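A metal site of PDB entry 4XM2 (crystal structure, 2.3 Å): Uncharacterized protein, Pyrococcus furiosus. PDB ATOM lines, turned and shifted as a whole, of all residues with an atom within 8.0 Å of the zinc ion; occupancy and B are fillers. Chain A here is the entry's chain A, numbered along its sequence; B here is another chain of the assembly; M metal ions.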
ATOM      1  N   GLU A  38      32.318  33.259  13.304  1.00  0.00           N
ATOM      2  CA  GLU A  38      31.657  32.413  12.285  1.00  0.00           C
ATOM      3  C   GLU A  38      31.006  31.167  12.901  1.00  0.00           C
ATOM      4  O   GLU A  38      31.547  30.603  13.838  1.00  0.00           O
ATOM      5  CB  GLU A  38      32.601  32.063  11.141  1.00  0.00           C
ATOM      6  CG  GLU A  38      34.095  31.932  11.532  1.00  0.00           C
ATOM      7  CD  GLU A  38      34.934  31.138  10.570  1.00  0.00           C
ATOM      8  OE1 GLU A  38      34.677  31.191   9.335  1.00  0.00           O
ATOM      9  OE2 GLU A  38      35.858  30.428  11.036  1.00  0.00           O
ATOM     10  N   PRO A  39      29.822  30.750  12.395  1.00  0.00           N
ATOM     11  CA  PRO A  39      29.192  29.473  12.827  1.00  0.00           C
ATOM     12  C   PRO A  39      30.033  28.251  12.504  1.00  0.00           C
ATOM     13  O   PRO A  39      30.178  27.345  13.363  1.00  0.00           O
ATOM     14  CB  PRO A  39      27.895  29.424  11.977  1.00  0.00           C
ATOM     15  CG  PRO A  39      27.611  30.844  11.696  1.00  0.00           C
ATOM     16  CD  PRO A  39      28.910  31.510  11.520  1.00  0.00           C
ATOM     17  N   HIS A  40      30.570  28.194  11.279  1.00  0.00           N
ATOM     18  CA  HIS A  40      31.381  27.047  10.806  1.00  0.00           C
ATOM     19  C   HIS A  40      32.628  27.538  10.139  1.00  0.00           C
ATOM     20  O   HIS A  40      32.639  28.690   9.649  1.00  0.00           O
ATOM     21  CB  HIS A  40      30.639  26.204   9.781  1.00  0.00           C
ATOM     22  CG  HIS A  40      29.247  25.845  10.161  1.00  0.00           C
ATOM     23  ND1 HIS A  40      28.155  26.341   9.505  1.00  0.00           N
ATOM     24  CD2 HIS A  40      28.771  25.006  11.124  1.00  0.00           C
ATOM     25  CE1 HIS A  40      27.051  25.852  10.052  1.00  0.00           C
ATOM     26  NE2 HIS A  40      27.401  25.020  11.022  1.00  0.00           N
ATOM     27  N   PRO A  41      33.676  26.692  10.053  1.00  0.00           N
ATOM     28  CA  PRO A  41      34.840  27.073   9.234  1.00  0.00           C
ATOM     29  C   PRO A  41      34.412  27.405   7.787  1.00  0.00           C
ATOM     30  O   PRO A  41      33.634  26.667   7.200  1.00  0.00           O
ATOM     31  CB  PRO A  41      35.706  25.794   9.256  1.00  0.00           C
ATOM     32  CG  PRO A  41      35.244  25.045  10.466  1.00  0.00           C
ATOM     33  CD  PRO A  41      33.768  25.278  10.466  1.00  0.00           C
ATOM     34  N   ASP A  42      34.895  28.527   7.244  1.00  0.00           N
ATOM     35  CA  ASP A  42      34.579  29.024   5.880  1.00  0.00           C
ATOM     36  C   ASP A  42      33.622  30.214   5.870  1.00  0.00           C
ATOM     37  O   ASP A  42      33.532  30.916   4.868  1.00  0.00           O
ATOM     38  CB  ASP A  42      34.156  27.915   4.858  1.00  0.00           C
ATOM     39  CG  ASP A  42      32.682  27.421   5.025  1.00  0.00           C
ATOM     40  OD1 ASP A  42      31.899  27.960   5.833  1.00  0.00           O
ATOM     41  OD2 ASP A  42      32.298  26.447   4.336  1.00  0.00           O
ATOM     42  N   ASP A  43      32.929  30.465   6.981  1.00  0.00           N
ATOM     43  CA  ASP A  43      31.853  31.484   6.946  1.00  0.00           C
ATOM     44  C   ASP A  43      32.421  32.903   6.938  1.00  0.00           C
ATOM     45  O   ASP A  43      31.906  33.758   6.248  1.00  0.00           O
ATOM     46  CB  ASP A  43      30.772  31.280   8.042  1.00  0.00           C
ATOM     47  CG  ASP A  43      29.718  30.244   7.666  1.00  0.00           C
ATOM     48  OD1 ASP A  43      29.121  30.343   6.595  1.00  0.00           O
ATOM     49  OD2 ASP A  43      29.410  29.307   8.467  1.00  0.00           O
ATOM     50  N   CYS A  44      33.444  33.147   7.728  1.00  0.00           N
ATOM     51  CA  CYS A  44      34.210  34.411   7.633  1.00  0.00           C
ATOM     52  C   CYS A  44      34.718  34.703   6.178  1.00  0.00           C
ATOM     53  O   CYS A  44      34.466  35.792   5.639  1.00  0.00           O
ATOM     54  CB  CYS A  44      35.387  34.375   8.577  1.00  0.00           C
ATOM     55  SG  CYS A  44      34.971  34.803  10.279  1.00  0.00           S
ATOM     56  N   ILE A  46      33.726  33.261   3.161  1.00  0.00           N
ATOM     57  CA  ILE A  46      32.563  33.478   2.302  1.00  0.00           C
ATOM     58  C   ILE A  46      31.841  34.797   2.502  1.00  0.00           C
ATOM     59  O   ILE A  46      31.402  35.419   1.530  1.00  0.00           O
ATOM     60  CB  ILE A  46      31.531  32.369   2.482  1.00  0.00           C
ATOM     61  CG1 ILE A  46      32.159  31.029   2.087  1.00  0.00           C
ATOM     62  CG2 ILE A  46      30.255  32.756   1.720  1.00  0.00           C
ATOM     63  CD1 ILE A  46      31.169  29.909   1.888  1.00  0.00           C
ATOM     64  N   THR A  68      31.653  26.431  15.882  1.00  0.00           N
ATOM     65  CA  THR A  68      31.516  24.973  15.799  1.00  0.00           C
ATOM     66  C   THR A  68      32.701  24.349  15.060  1.00  0.00           C
ATOM     67  O   THR A  68      33.560  25.065  14.579  1.00  0.00           O
ATOM     68  CB  THR A  68      30.228  24.479  15.068  1.00  0.00           C
ATOM     69  OG1 THR A  68      30.228  24.943  13.721  1.00  0.00           O
ATOM     70  CG2 THR A  68      28.926  24.937  15.737  1.00  0.00           C
ATOM     71  N   ARG A  88      39.045  20.255   8.738  1.00  0.00           N
ATOM     72  CA  ARG A  88      38.469  21.561   8.523  1.00  0.00           C
ATOM     73  C   ARG A  88      39.210  22.634   9.260  1.00  0.00           C
ATOM     74  O   ARG A  88      39.158  23.797   8.846  1.00  0.00           O
ATOM     75  CB  ARG A  88      36.965  21.573   8.771  1.00  0.00           C
ATOM     76  CG  ARG A  88      36.235  20.943   7.582  1.00  0.00           C
ATOM     77  CD  ARG A  88      34.763  21.126   7.649  1.00  0.00           C
ATOM     78  NE  ARG A  88      34.324  22.480   7.359  1.00  0.00           N
ATOM     79  CZ  ARG A  88      33.042  22.803   7.279  1.00  0.00           C
ATOM     80  NH1 ARG A  88      32.150  21.859   7.506  1.00  0.00           N
ATOM     81  NH2 ARG A  88      32.633  24.040   6.985  1.00  0.00           N
ATOM     82  N   ASP A 111      29.066  21.162  15.112  1.00  0.00           N
ATOM     83  CA  ASP A 111      28.241  21.455  13.938  1.00  0.00           C
ATOM     84  C   ASP A 111      26.840  20.851  14.072  1.00  0.00           C
ATOM     85  O   ASP A 111      26.697  19.675  14.360  1.00  0.00           O
ATOM     86  CB  ASP A 111      29.014  20.940  12.704  1.00  0.00           C
ATOM     87  CG  ASP A 111      28.340  21.229  11.360  1.00  0.00           C
ATOM     88  OD1 ASP A 111      27.407  22.063  11.223  1.00  0.00           O
ATOM     89  OD2 ASP A 111      28.835  20.603  10.408  1.00  0.00           O
ATOM     90  N   PRO A 139      27.072  37.102  11.513  1.00  0.00           N
ATOM     91  CA  PRO A 139      25.962  37.017  10.549  1.00  0.00           C
ATOM     92  C   PRO A 139      24.771  37.724  11.117  1.00  0.00           C
ATOM     93  O   PRO A 139      24.643  37.777  12.335  1.00  0.00           O
ATOM     94  CB  PRO A 139      25.642  35.504  10.493  1.00  0.00           C
ATOM     95  CG  PRO A 139      26.928  34.833  11.149  1.00  0.00           C
ATOM     96  CD  PRO A 139      27.322  35.795  12.166  1.00  0.00           C
ATOM     97  N   GLU A 146      16.812  32.034   6.236  1.00  0.00           N
ATOM     98  CA  GLU A 146      17.998  31.341   6.711  1.00  0.00           C
ATOM     99  C   GLU A 146      17.587  30.177   7.580  1.00  0.00           C
ATOM    100  O   GLU A 146      16.958  30.388   8.598  1.00  0.00           O
ATOM    101  CB  GLU A 146      18.916  32.241   7.534  1.00  0.00           C
ATOM    102  CG  GLU A 146      20.021  31.443   8.213  1.00  0.00           C
ATOM    103  CD  GLU A 146      20.995  30.773   7.226  1.00  0.00           C
ATOM    104  OE1 GLU A 146      21.187  29.517   7.302  1.00  0.00           O
ATOM    105  OE2 GLU A 146      21.642  31.511   6.433  1.00  0.00           O
ATOM    106  N   HIS A 148      19.731  27.403   8.734  1.00  0.00           N
ATOM    107  CA  HIS A 148      20.674  26.765   9.575  1.00  0.00           C
ATOM    108  C   HIS A 148      20.635  27.280  11.067  1.00  0.00           C
ATOM    109  O   HIS A 148      21.155  28.339  11.388  1.00  0.00           O
ATOM    110  CB  HIS A 148      22.070  26.912   9.016  1.00  0.00           C
ATOM    111  CG  HIS A 148      22.971  25.778   9.386  1.00  0.00           C
ATOM    112  ND1 HIS A 148      23.670  25.046   8.444  1.00  0.00           N
ATOM    113  CD2 HIS A 148      23.214  25.200  10.590  1.00  0.00           C
ATOM    114  CE1 HIS A 148      24.346  24.090   9.075  1.00  0.00           C
ATOM    115  NE2 HIS A 148      24.088  24.165  10.367  1.00  0.00           N
ATOM    116  N   ASP A 150      22.651  26.826  13.522  1.00  0.00           N
ATOM    117  CA  ASP A 150      23.953  27.414  13.887  1.00  0.00           C
ATOM    118  C   ASP A 150      24.157  28.881  13.405  1.00  0.00           C
ATOM    119  O   ASP A 150      24.868  29.656  14.030  1.00  0.00           O
ATOM    120  CB  ASP A 150      25.131  26.608  13.315  1.00  0.00           C
ATOM    121  CG  ASP A 150      25.162  25.136  13.778  1.00  0.00           C
ATOM    122  OD1 ASP A 150      24.419  24.762  14.732  1.00  0.00           O
ATOM    123  OD2 ASP A 150      25.970  24.340  13.197  1.00  0.00           O
ATOM    124  N   HIS A 151      23.596  29.267  12.275  1.00  0.00           N
ATOM    125  CA  HIS A 151      23.874  30.630  11.785  1.00  0.00           C
ATOM    126  C   HIS A 151      23.015  31.630  12.518  1.00  0.00           C
ATOM    127  O   HIS A 151      23.496  32.708  12.894  1.00  0.00           O
ATOM    128  CB  HIS A 151      23.556  30.754  10.313  1.00  0.00           C
ATOM    129  CG  HIS A 151      24.662  30.345   9.430  1.00  0.00           C
ATOM    130  ND1 HIS A 151      25.212  31.190   8.479  1.00  0.00           N
ATOM    131  CD2 HIS A 151      25.292  29.156   9.287  1.00  0.00           C
ATOM    132  CE1 HIS A 151      26.160  30.543   7.831  1.00  0.00           C
ATOM    133  NE2 HIS A 151      26.217  29.312   8.296  1.00  0.00           N
ATOM    134  N   THR A 154      24.273  31.848  16.064  1.00  0.00           N
ATOM    135  CA  THR A 154      25.543  32.590  16.138  1.00  0.00           C
ATOM    136  C   THR A 154      25.316  34.110  16.120  1.00  0.00           C
ATOM    137  O   THR A 154      25.827  34.858  16.986  1.00  0.00           O
ATOM    138  CB  THR A 154      26.477  32.182  14.987  1.00  0.00           C
ATOM    139  OG1 THR A 154      26.870  30.802  15.137  1.00  0.00           O
ATOM    140  CG2 THR A 154      27.777  33.065  14.953  1.00  0.00           C
ATOM    141  N   TYR A 191      26.336  38.593   5.851  1.00  0.00           N
ATOM    142  CA  TYR A 191      25.249  37.781   5.356  1.00  0.00           C
ATOM    143  C   TYR A 191      23.925  38.514   5.566  1.00  0.00           C
ATOM    144  O   TYR A 191      22.971  37.912   6.080  1.00  0.00           O
ATOM    145  CB  TYR A 191      25.185  36.453   6.103  1.00  0.00           C
ATOM    146  CG  TYR A 191      26.225  35.416   5.760  1.00  0.00           C
ATOM    147  CD1 TYR A 191      26.605  35.179   4.458  1.00  0.00           C
ATOM    148  CD2 TYR A 191      26.775  34.621   6.747  1.00  0.00           C
ATOM    149  CE1 TYR A 191      27.549  34.165   4.141  1.00  0.00           C
ATOM    150  CE2 TYR A 191      27.720  33.592   6.460  1.00  0.00           C
ATOM    151  CZ  TYR A 191      28.096  33.378   5.142  1.00  0.00           C
ATOM    152  OH  TYR A 191      29.006  32.380   4.822  1.00  0.00           O
ATOM    153  N   HIS B 259      19.848  29.037   2.681  1.00  0.00           N
ATOM    154  CA  HIS B 259      21.093  29.305   3.397  1.00  0.00           C
ATOM    155  C   HIS B 259      21.756  30.574   2.825  1.00  0.00           C
ATOM    156  O   HIS B 259      21.831  30.744   1.609  1.00  0.00           O
ATOM    157  CB  HIS B 259      22.021  28.084   3.281  1.00  0.00           C
ATOM    158  CG  HIS B 259      23.146  28.040   4.280  1.00  0.00           C
ATOM    159  ND1 HIS B 259      22.954  28.219   5.641  1.00  0.00           N
ATOM    160  CD2 HIS B 259      24.465  27.772   4.120  1.00  0.00           C
ATOM    161  CE1 HIS B 259      24.115  28.103   6.263  1.00  0.00           C
ATOM    162  NE2 HIS B 259      25.040  27.807   5.373  1.00  0.00           N
ATOM    163  N   ILE B 260      22.244  31.432   3.735  1.00  0.00           N
ATOM    164  CA  ILE B 260      23.082  32.582   3.394  1.00  0.00           C
ATOM    165  C   ILE B 260      22.754  33.226   2.020  1.00  0.00           C
ATOM    166  O   ILE B 260      23.655  33.617   1.300  1.00  0.00           O
ATOM    167  CB  ILE B 260      24.609  32.233   3.526  1.00  0.00           C
ATOM    168  CG1 ILE B 260      25.096  31.225   2.457  1.00  0.00           C
ATOM    169  CG2 ILE B 260      24.939  31.719   4.925  1.00  0.00           C
ATOM    170  CD1 ILE B 260      26.567  30.742   2.666  1.00  0.00           C
HETATM  171 ZN    ZN M   1      28.003  27.985   7.904  1.00  0.00          ZN
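N of Asp 43 lies within hydrogen-bond range of OE1 of Glu 38. NE2 of His 40 lies within hydrogen-bond range of OD1 of Asp 111, at 3.0 Å. The side-chain carboxylate of Glu 146 is in hydrogen-bond range of a ring nitrogen (ND1) of His 259 of chain B (2.8 Å). The side-chain carboxylate of Asp 43 lies within hydrogen-bond range of the side-chain hydroxyl of Tyr 191 (2.7 Å). NE2 of His 151 lies close to NE2 of His 259 of chain B (3.5 Å). NE2 of His 40 sits at hydrogen-bond distance from OD2 of Asp 150, at 2.7 Å. A ring nitrogen (NE2) of His 40 sits close to a ring nitrogen (NE2) of His 148 (3.5 Å).
NE2 of His 259 of chain B touches the zinc ion (3.9 Å). Of the 20 residues printed, 4 come within 4 Å of the zinc ion.
The zinc ion is bound by OD2 of Asp 43. The zinc ion is bound by a ring nitrogen (NE2) of His 151 (2.3 Å). The zinc ion is bound by ND1 of His 40 (2.3 Å).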
